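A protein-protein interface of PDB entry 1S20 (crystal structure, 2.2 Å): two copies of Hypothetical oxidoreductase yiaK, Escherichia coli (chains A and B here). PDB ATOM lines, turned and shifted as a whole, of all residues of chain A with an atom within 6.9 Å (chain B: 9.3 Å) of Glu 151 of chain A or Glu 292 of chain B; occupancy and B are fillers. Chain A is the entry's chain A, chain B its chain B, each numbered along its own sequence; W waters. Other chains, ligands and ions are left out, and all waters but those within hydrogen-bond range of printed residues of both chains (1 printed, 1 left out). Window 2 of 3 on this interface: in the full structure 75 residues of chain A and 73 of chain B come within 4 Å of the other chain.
Printed residues of chain A that touch a printed residue of chain B: Pro 146, Gly 148, Ala 149, Lys 150, Glu 151, Arg 153, Ile 154 and Arg 217.
Hydrophobic or aromatic side chains of chain A within 4 Å of the printed part of chain B: Pro 146, Ala 149 and Ile 154.
Of the 14 printed residues of chain B, 8 touch a printed residue of chain A.
Hydrophobic or aromatic side chains of chain B that line the printed part of chain A: Tyr 287, Val 288, Ala 291, Ala 294 and Ile 300.
Water W1 bridges NH1 of Arg 217 of chain A (2.8 Å) and O of Ala 294 of chain B (3.5 Å).
O of Met 144 of chain A lies within hydrogen-bond range of N of Ile 154 of chain A (2.8 Å).
OG of Ser 290 of chain B lies within hydrogen-bond range of O of Asp 286 of chain B, at 2.6 Å.
The guanidinium group of Arg 293 of chain B sits at hydrogen-bond distance from the backbone carbonyl oxygen of Glu 296 of chain B, 3.0 Å away.
The backbone carbonyl oxygen of Met 144 of chain A is in hydrogen-bond range of the backbone NH of Arg 153 of chain A.
The guanidinium group of Arg 153 of chain A lies within salt-bridge range of the side-chain carboxylate of Glu 151 of chain A, 2.7 Å away.
OD1 of Asn 215 of chain A sits at hydrogen-bond distance from N of Arg 217 of chain A (2.8 Å).
Ala 142 of chain A touches none of the printed residues of chain B.
Lys 150 of chain A touches just these residues of chain B: Glu 292 and Arg 293.
Of chain B, only Ala 291 and Glu 292 come within 4 Å of Glu 151 of chain A.
No residue of chain B comes within 4 Å of Cys 152 of chain A.
Printed residues of chain A within 4 Å of Tyr 287 of chain B: Arg 153.
Printed residues of chain A within 4 Å of Glu 292 of chain B: Ala 149, Lys 150 and Glu 151.
Of the printed residues of chain A, Ala 294 of chain B touches Gly 148, Ala 149 and Arg 217.
The nearest residue of chain A that does not touch Glu 292 of chain B is Gly 148 of chain A (4.8 Å).
The nearest printed residue of chain A that does not touch Tyr 287 of chain B is Ala 142 of chain A (4.0005 Å).
The backbone carbonyl oxygen (O) of Gly 148 of chain A lies within hydrogen-bond range of the backbone NH (N) of Ala 294 of chain B (2.9 Å).
NH1 of Arg 153 of chain A lies within hydrogen-bond range of O of Tyr 287 of chain B, 3.0 Å away.
The side-chain carboxylate (OE1) of Glu 151 of chain A lies within hydrogen-bond range of the backbone NH (N) of Glu 292 of chain B.
The backbone carbonyl oxygen of Glu 292 of chain B is in hydrogen-bond range of the backbone NH of Lys 150 of chain A (2.9 Å).
The guanidinium group (NH1) of Arg 153 of chain A is in hydrogen-bond range of the side-chain hydroxyl (OG) of Ser 290 of chain B (3.2 Å).
Among the printed residues, merely in contact across the chains: Pro 146 of chain A with Val 288 of chain B (3.8 Å), Gly 148 of chain A with Arg 293 of chain B (3.7 Å), Gly 148 of chain A with Ile 300 of chain B (3.9 Å), Ala 149 of chain A with Ala 291 of chain B (3.8 Å), Ala 149 of chain A with Glu 292 of chain B (3.4 Å), Ala 149 of chain A with Ala 294 of chain B (3.9 Å), Ala 149 of chain A with Ile 300 of chain B (3.6 Å), Lys 150 of chain A with Arg 293 of chain B (3.6 Å), Glu 151 of chain A with Ala 291 of chain B (3.5 Å), Arg 153 of chain A with Ala 291 of chain B (3.5 Å), Ile 154 of chain A with Val 288 of chain B (3.96 Å) and Arg 217 of chain A with Ala 294 of chain B (3.7 Å).
No position is printed for both chains.
Of the 17 pairs that touch across the chains among the printed residues, none has its exchanged pair printed and touching as well.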
ATOM      1  N   ALA A 142       0.474 -10.366 -17.797  1.00  0.00           N
ATOM      2  CA  ALA A 142       0.900  -9.025 -18.160  1.00  0.00           C
ATOM      3  C   ALA A 142       0.172  -8.606 -19.430  1.00  0.00           C
ATOM      4  O   ALA A 142       0.436  -9.134 -20.507  1.00  0.00           O
ATOM      5  CB  ALA A 142       2.397  -9.002 -18.379  1.00  0.00           C
ATOM      6  N   MET A 144      -0.555  -5.089 -19.661  1.00  0.00           N
ATOM      7  CA  MET A 144      -0.361  -3.651 -19.596  1.00  0.00           C
ATOM      8  C   MET A 144       1.088  -3.291 -19.285  1.00  0.00           C
ATOM      9  O   MET A 144       1.726  -3.912 -18.428  1.00  0.00           O
ATOM     10  CB  MET A 144      -1.285  -3.044 -18.535  1.00  0.00           C
ATOM     11  CG  MET A 144      -1.000  -1.584 -18.196  1.00  0.00           C
ATOM     12  SD  MET A 144      -2.387  -0.750 -17.105  1.00  0.00           S
ATOM     13  CE  MET A 144      -2.374  -1.904 -15.548  1.00  0.00           C
ATOM     14  N   PRO A 145       1.628  -2.287 -19.989  1.00  0.00           N
ATOM     15  CA  PRO A 145       3.008  -1.859 -19.766  1.00  0.00           C
ATOM     16  C   PRO A 145       3.117  -0.922 -18.570  1.00  0.00           C
ATOM     17  O   PRO A 145       2.287  -0.019 -18.393  1.00  0.00           O
ATOM     18  CB  PRO A 145       3.360  -1.159 -21.074  1.00  0.00           C
ATOM     19  CG  PRO A 145       2.063  -0.536 -21.452  1.00  0.00           C
ATOM     20  CD  PRO A 145       1.071  -1.646 -21.191  1.00  0.00           C
ATOM     21  N   PRO A 146       4.129  -1.137 -17.714  1.00  0.00           N
ATOM     22  CA  PRO A 146       4.338  -0.290 -16.534  1.00  0.00           C
ATOM     23  C   PRO A 146       4.626   1.123 -17.023  1.00  0.00           C
ATOM     24  O   PRO A 146       5.037   1.310 -18.174  1.00  0.00           O
ATOM     25  CB  PRO A 146       5.537  -0.944 -15.851  1.00  0.00           C
ATOM     26  CG  PRO A 146       6.299  -1.517 -16.995  1.00  0.00           C
ATOM     27  CD  PRO A 146       5.207  -2.130 -17.841  1.00  0.00           C
ATOM     28  N   GLY A 148       6.193   4.272 -18.198  1.00  0.00           N
ATOM     29  CA  GLY A 148       7.520   4.522 -18.725  1.00  0.00           C
ATOM     30  C   GLY A 148       7.870   3.480 -19.772  1.00  0.00           C
ATOM     31  O   GLY A 148       8.866   3.638 -20.469  1.00  0.00           O
ATOM     32  N   ALA A 149       7.061   2.424 -19.892  1.00  0.00           N
ATOM     33  CA  ALA A 149       7.305   1.364 -20.879  1.00  0.00           C
ATOM     34  C   ALA A 149       6.274   1.332 -22.011  1.00  0.00           C
ATOM     35  O   ALA A 149       5.272   2.050 -21.980  1.00  0.00           O
ATOM     36  CB  ALA A 149       7.329   0.006 -20.191  1.00  0.00           C
ATOM     37  N   LYS A 150       6.536   0.493 -23.011  1.00  0.00           N
ATOM     38  CA  LYS A 150       5.636   0.321 -24.144  1.00  0.00           C
ATOM     39  C   LYS A 150       5.379  -1.165 -24.305  1.00  0.00           C
ATOM     40  O   LYS A 150       4.665  -1.579 -25.213  1.00  0.00           O
ATOM     41  CB  LYS A 150       6.251   0.856 -25.438  1.00  0.00           C
ATOM     42  CG  LYS A 150       7.477   0.075 -25.893  1.00  0.00           C
ATOM     43  CD  LYS A 150       7.868   0.375 -27.339  1.00  0.00           C
ATOM     44  CE  LYS A 150       8.290   1.821 -27.552  1.00  0.00           C
ATOM     45  NZ  LYS A 150       8.992   1.960 -28.860  1.00  0.00           N
ATOM     46  N   GLU A 151       5.974  -1.965 -23.423  1.00  0.00           N
ATOM     47  CA  GLU A 151       5.815  -3.418 -23.455  1.00  0.00           C
ATOM     48  C   GLU A 151       5.044  -3.870 -22.218  1.00  0.00           C
ATOM     49  O   GLU A 151       5.380  -3.486 -21.097  1.00  0.00           O
ATOM     50  CB  GLU A 151       7.192  -4.100 -23.503  1.00  0.00           C
ATOM     51  CG  GLU A 151       7.148  -5.621 -23.310  1.00  0.00           C
ATOM     52  CD  GLU A 151       8.514  -6.302 -23.469  1.00  0.00           C
ATOM     53  OE1 GLU A 151       9.538  -5.719 -23.042  1.00  0.00           O
ATOM     54  OE2 GLU A 151       8.557  -7.428 -24.018  1.00  0.00           O
ATOM     55  N   CYS A 152       4.004  -4.676 -22.416  1.00  0.00           N
ATOM     56  CA  CYS A 152       3.201  -5.150 -21.288  1.00  0.00           C
ATOM     57  C   CYS A 152       4.008  -6.042 -20.356  1.00  0.00           C
ATOM     58  O   CYS A 152       4.527  -7.085 -20.764  1.00  0.00           O
ATOM     59  CB  CYS A 152       1.963  -5.908 -21.782  1.00  0.00           C
ATOM     60  SG  CYS A 152       0.789  -4.887 -22.719  1.00  0.00           S
ATOM     61  N   ARG A 153       4.111  -5.618 -19.099  1.00  0.00           N
ATOM     62  CA  ARG A 153       4.839  -6.376 -18.098  1.00  0.00           C
ATOM     63  C   ARG A 153       4.125  -6.362 -16.757  1.00  0.00           C
ATOM     64  O   ARG A 153       4.642  -6.901 -15.777  1.00  0.00           O
ATOM     65  CB  ARG A 153       6.263  -5.833 -17.946  1.00  0.00           C
ATOM     66  CG  ARG A 153       7.178  -6.138 -19.135  1.00  0.00           C
ATOM     67  CD  ARG A 153       7.338  -7.639 -19.351  1.00  0.00           C
ATOM     68  NE  ARG A 153       8.152  -7.937 -20.529  1.00  0.00           N
ATOM     69  CZ  ARG A 153       9.471  -7.771 -20.596  1.00  0.00           C
ATOM     70  NH1 ARG A 153      10.139  -7.314 -19.547  1.00  0.00           N
ATOM     71  NH2 ARG A 153      10.120  -8.049 -21.721  1.00  0.00           N
ATOM     72  N   ILE A 154       2.953  -5.730 -16.707  1.00  0.00           N
ATOM     73  CA  ILE A 154       2.171  -5.702 -15.469  1.00  0.00           C
ATOM     74  C   ILE A 154       0.715  -6.113 -15.719  1.00  0.00           C
ATOM     75  O   ILE A 154       0.227  -6.037 -16.849  1.00  0.00           O
ATOM     76  CB  ILE A 154       2.212  -4.302 -14.782  1.00  0.00           C
ATOM     77  CG1 ILE A 154       1.490  -3.264 -15.634  1.00  0.00           C
ATOM     78  CG2 ILE A 154       3.677  -3.854 -14.565  1.00  0.00           C
ATOM     79  CD1 ILE A 154       1.442  -1.923 -14.982  1.00  0.00           C
ATOM     80  N   ASN A 215      -1.698  -2.112 -30.236  1.00  0.00           N
ATOM     81  CA  ASN A 215      -0.360  -2.112 -29.659  1.00  0.00           C
ATOM     82  C   ASN A 215      -0.341  -2.576 -28.206  1.00  0.00           C
ATOM     83  O   ASN A 215       0.722  -2.778 -27.631  1.00  0.00           O
ATOM     84  CB  ASN A 215       0.287  -0.724 -29.770  1.00  0.00           C
ATOM     85  CG  ASN A 215      -0.593   0.383 -29.222  1.00  0.00           C
ATOM     86  OD1 ASN A 215      -1.337   0.185 -28.260  1.00  0.00           O
ATOM     87  ND2 ASN A 215      -0.496   1.565 -29.827  1.00  0.00           N
ATOM     88  N   ARG A 216      -1.520  -2.756 -27.621  1.00  0.00           N
ATOM     89  CA  ARG A 216      -1.629  -3.201 -26.235  1.00  0.00           C
ATOM     90  C   ARG A 216      -1.049  -2.186 -25.251  1.00  0.00           C
ATOM     91  O   ARG A 216      -0.742  -2.528 -24.110  1.00  0.00           O
ATOM     92  CB  ARG A 216      -0.923  -4.545 -26.057  1.00  0.00           C
ATOM     93  CG  ARG A 216      -1.220  -5.547 -27.170  1.00  0.00           C
ATOM     94  CD  ARG A 216      -2.701  -5.725 -27.361  1.00  0.00           C
ATOM     95  NE  ARG A 216      -3.328  -6.381 -26.217  1.00  0.00           N
ATOM     96  CZ  ARG A 216      -4.638  -6.585 -26.102  1.00  0.00           C
ATOM     97  NH1 ARG A 216      -5.129  -7.199 -25.027  1.00  0.00           N
ATOM     98  NH2 ARG A 216      -5.456  -6.156 -27.060  1.00  0.00           N
ATOM     99  N   ARG A 217      -0.890  -0.943 -25.689  1.00  0.00           N
ATOM    100  CA  ARG A 217      -0.348   0.086 -24.807  1.00  0.00           C
ATOM    101  C   ARG A 217      -1.490   0.740 -24.027  1.00  0.00           C
ATOM    102  O   ARG A 217      -1.694   1.948 -24.085  1.00  0.00           O
ATOM    103  CB  ARG A 217       0.431   1.142 -25.613  1.00  0.00           C
ATOM    104  CG  ARG A 217       1.722   0.606 -26.243  1.00  0.00           C
ATOM    105  CD  ARG A 217       2.564   1.687 -26.918  1.00  0.00           C
ATOM    106  NE  ARG A 217       3.194   2.585 -25.949  1.00  0.00           N
ATOM    107  CZ  ARG A 217       4.033   3.573 -26.255  1.00  0.00           C
ATOM    108  NH1 ARG A 217       4.364   3.813 -27.521  1.00  0.00           N
ATOM    109  NH2 ARG A 217       4.536   4.327 -25.282  1.00  0.00           N
ATOM    110  N   ASP B 286      12.540  -6.991 -12.020  1.00  0.00           N
ATOM    111  CA  ASP B 286      13.269  -6.995 -13.292  1.00  0.00           C
ATOM    112  C   ASP B 286      12.319  -7.115 -14.471  1.00  0.00           C
ATOM    113  O   ASP B 286      12.597  -6.612 -15.560  1.00  0.00           O
ATOM    114  CB  ASP B 286      14.272  -8.151 -13.343  1.00  0.00           C
ATOM    115  CG  ASP B 286      15.282  -8.089 -12.227  1.00  0.00           C
ATOM    116  OD1 ASP B 286      15.557  -6.976 -11.739  1.00  0.00           O
ATOM    117  OD2 ASP B 286      15.809  -9.153 -11.846  1.00  0.00           O
ATOM    118  N   TYR B 287      11.194  -7.780 -14.252  1.00  0.00           N
ATOM    119  CA  TYR B 287      10.219  -7.949 -15.314  1.00  0.00           C
ATOM    120  C   TYR B 287       9.690  -6.579 -15.704  1.00  0.00           C
ATOM    121  O   TYR B 287       9.310  -6.351 -16.857  1.00  0.00           O
ATOM    122  CB  TYR B 287       9.070  -8.831 -14.842  1.00  0.00           C
ATOM    123  CG  TYR B 287       8.212  -9.363 -15.959  1.00  0.00           C
ATOM    124  CD1 TYR B 287       6.830  -9.248 -15.904  1.00  0.00           C
ATOM    125  CD2 TYR B 287       8.777 -10.045 -17.037  1.00  0.00           C
ATOM    126  CE1 TYR B 287       6.023  -9.802 -16.885  1.00  0.00           C
ATOM    127  CE2 TYR B 287       7.981 -10.609 -18.030  1.00  0.00           C
ATOM    128  CZ  TYR B 287       6.600 -10.487 -17.944  1.00  0.00           C
ATOM    129  OH  TYR B 287       5.781 -11.075 -18.884  1.00  0.00           O
ATOM    130  N   VAL B 288       9.679  -5.669 -14.729  1.00  0.00           N
ATOM    131  CA  VAL B 288       9.216  -4.302 -14.937  1.00  0.00           C
ATOM    132  C   VAL B 288      10.323  -3.412 -15.500  1.00  0.00           C
ATOM    133  O   VAL B 288      10.123  -2.731 -16.493  1.00  0.00           O
ATOM    134  CB  VAL B 288       8.711  -3.655 -13.607  1.00  0.00           C
ATOM    135  CG1 VAL B 288       8.550  -2.145 -13.784  1.00  0.00           C
ATOM    136  CG2 VAL B 288       7.375  -4.271 -13.203  1.00  0.00           C
ATOM    137  N   THR B 289      11.483  -3.412 -14.856  1.00  0.00           N
ATOM    138  CA  THR B 289      12.595  -2.574 -15.286  1.00  0.00           C
ATOM    139  C   THR B 289      13.278  -2.969 -16.595  1.00  0.00           C
ATOM    140  O   THR B 289      14.061  -2.190 -17.141  1.00  0.00           O
ATOM    141  CB  THR B 289      13.666  -2.472 -14.164  1.00  0.00           C
ATOM    142  OG1 THR B 289      14.152  -3.777 -13.829  1.00  0.00           O
ATOM    143  CG2 THR B 289      13.071  -1.826 -12.920  1.00  0.00           C
ATOM    144  N   SER B 290      12.995  -4.166 -17.102  1.00  0.00           N
ATOM    145  CA  SER B 290      13.608  -4.590 -18.359  1.00  0.00           C
ATOM    146  C   SER B 290      12.673  -4.431 -19.553  1.00  0.00           C
ATOM    147  O   SER B 290      13.039  -4.773 -20.675  1.00  0.00           O
ATOM    148  CB  SER B 290      14.060  -6.047 -18.272  1.00  0.00           C
ATOM    149  OG  SER B 290      12.947  -6.914 -18.133  1.00  0.00           O
ATOM    150  N   ALA B 291      11.472  -3.915 -19.307  1.00  0.00           N
ATOM    151  CA  ALA B 291      10.491  -3.724 -20.374  1.00  0.00           C
ATOM    152  C   ALA B 291      10.953  -2.686 -21.390  1.00  0.00           C
ATOM    153  O   ALA B 291      11.637  -1.735 -21.037  1.00  0.00           O
ATOM    154  CB  ALA B 291       9.144  -3.311 -19.783  1.00  0.00           C
ATOM    155  N   GLU B 292      10.583  -2.870 -22.652  1.00  0.00           N
ATOM    156  CA  GLU B 292      10.973  -1.927 -23.695  1.00  0.00           C
ATOM    157  C   GLU B 292      10.486  -0.537 -23.290  1.00  0.00           C
ATOM    158  O   GLU B 292       9.289  -0.319 -23.115  1.00  0.00           O
ATOM    159  CB  GLU B 292      10.360  -2.334 -25.038  1.00  0.00           C
ATOM    160  CG  GLU B 292      11.016  -1.652 -26.232  1.00  0.00           C
ATOM    161  CD  GLU B 292      10.340  -1.961 -27.558  1.00  0.00           C
ATOM    162  OE1 GLU B 292      10.897  -1.561 -28.604  1.00  0.00           O
ATOM    163  OE2 GLU B 292       9.259  -2.593 -27.559  1.00  0.00           O
ATOM    164  N   ARG B 293      11.421   0.391 -23.130  1.00  0.00           N
ATOM    165  CA  ARG B 293      11.104   1.751 -22.708  1.00  0.00           C
ATOM    166  C   ARG B 293      10.382   2.613 -23.741  1.00  0.00           C
ATOM    167  O   ARG B 293      10.609   2.484 -24.939  1.00  0.00           O
ATOM    168  CB  ARG B 293      12.390   2.459 -22.287  1.00  0.00           C
ATOM    169  CG  ARG B 293      13.200   1.698 -21.263  1.00  0.00           C
ATOM    170  CD  ARG B 293      14.548   2.355 -21.059  1.00  0.00           C
ATOM    171  NE  ARG B 293      15.338   1.660 -20.053  1.00  0.00           N
ATOM    172  CZ  ARG B 293      16.529   2.065 -19.630  1.00  0.00           C
ATOM    173  NH1 ARG B 293      17.076   3.165 -20.127  1.00  0.00           N
ATOM    174  NH2 ARG B 293      17.167   1.375 -18.700  1.00  0.00           N
ATOM    175  N   ALA B 294       9.511   3.500 -23.269  1.00  0.00           N
ATOM    176  CA  ALA B 294       8.790   4.398 -24.167  1.00  0.00           C
ATOM    177  C   ALA B 294       9.795   5.415 -24.691  1.00  0.00           C
ATOM    178  O   ALA B 294       9.705   5.866 -25.834  1.00  0.00           O
ATOM    179  CB  ALA B 294       7.667   5.105 -23.423  1.00  0.00           C
ATOM    180  N   ASP B 295      10.742   5.766 -23.824  1.00  0.00           N
ATOM    181  CA  ASP B 295      11.820   6.708 -24.122  1.00  0.00           C
ATOM    182  C   ASP B 295      13.103   6.020 -23.648  1.00  0.00           C
ATOM    183  O   ASP B 295      13.314   5.835 -22.446  1.00  0.00           O
ATOM    184  CB  ASP B 295      11.610   8.015 -23.352  1.00  0.00           C
ATOM    185  CG  ASP B 295      12.570   9.125 -23.785  1.00  0.00           C
ATOM    186  OD1 ASP B 295      13.792   8.881 -23.880  1.00  0.00           O
ATOM    187  OD2 ASP B 295      12.097  10.258 -24.022  1.00  0.00           O
ATOM    188  N   GLU B 296      13.947   5.643 -24.604  1.00  0.00           N
ATOM    189  CA  GLU B 296      15.200   4.947 -24.328  1.00  0.00           C
ATOM    190  C   GLU B 296      16.083   5.646 -23.304  1.00  0.00           C
ATOM    191  O   GLU B 296      16.749   4.992 -22.506  1.00  0.00           O
ATOM    192  CB  GLU B 296      15.983   4.753 -25.625  1.00  0.00           C
ATOM    193  CG  GLU B 296      17.067   3.704 -25.530  1.00  0.00           C
ATOM    194  CD  GLU B 296      16.525   2.369 -25.060  1.00  0.00           C
ATOM    195  OE1 GLU B 296      15.425   1.991 -25.517  1.00  0.00           O
ATOM    196  OE2 GLU B 296      17.196   1.701 -24.242  1.00  0.00           O
ATOM    197  N   GLN B 298      14.973   7.582 -20.936  1.00  0.00           N
ATOM    198  CA  GLN B 298      14.263   7.518 -19.665  1.00  0.00           C
ATOM    199  C   GLN B 298      14.087   6.064 -19.245  1.00  0.00           C
ATOM    200  O   GLN B 298      13.376   5.308 -19.901  1.00  0.00           O
ATOM    201  CB  GLN B 298      12.887   8.174 -19.792  1.00  0.00           C
ATOM    202  CG  GLN B 298      12.787   9.597 -19.243  1.00  0.00           C
ATOM    203  CD  GLN B 298      12.839   9.647 -17.721  1.00  0.00           C
ATOM    204  OE1 GLN B 298      13.906   9.486 -17.111  1.00  0.00           O
ATOM    205  NE2 GLN B 298      11.679   9.865 -17.099  1.00  0.00           N
ATOM    206  N   ALA B 299      14.734   5.675 -18.151  1.00  0.00           N
ATOM    207  CA  ALA B 299      14.631   4.304 -17.665  1.00  0.00           C
ATOM    208  C   ALA B 299      13.356   4.103 -16.857  1.00  0.00           C
ATOM    209  O   ALA B 299      12.854   5.036 -16.240  1.00  0.00           O
ATOM    210  CB  ALA B 299      15.844   3.956 -16.816  1.00  0.00           C
ATOM    211  N   ILE B 300      12.838   2.880 -16.874  1.00  0.00           N
ATOM    212  CA  ILE B 300      11.623   2.544 -16.145  1.00  0.00           C
ATOM    213  C   ILE B 300      11.953   2.434 -14.670  1.00  0.00           C
ATOM    214  O   ILE B 300      12.933   1.792 -14.296  1.00  0.00           O
ATOM    215  CB  ILE B 300      11.047   1.206 -16.622  1.00  0.00           C
ATOM    216  CG1 ILE B 300      10.896   1.232 -18.144  1.00  0.00           C
ATOM    217  CG2 ILE B 300       9.690   0.957 -15.967  1.00  0.00           C
ATOM    218  CD1 ILE B 300      10.577  -0.101 -18.743  1.00  0.00           C
HETATM  219  O   HOH W   1       6.628   5.391 -27.375  1.00  0.00           O
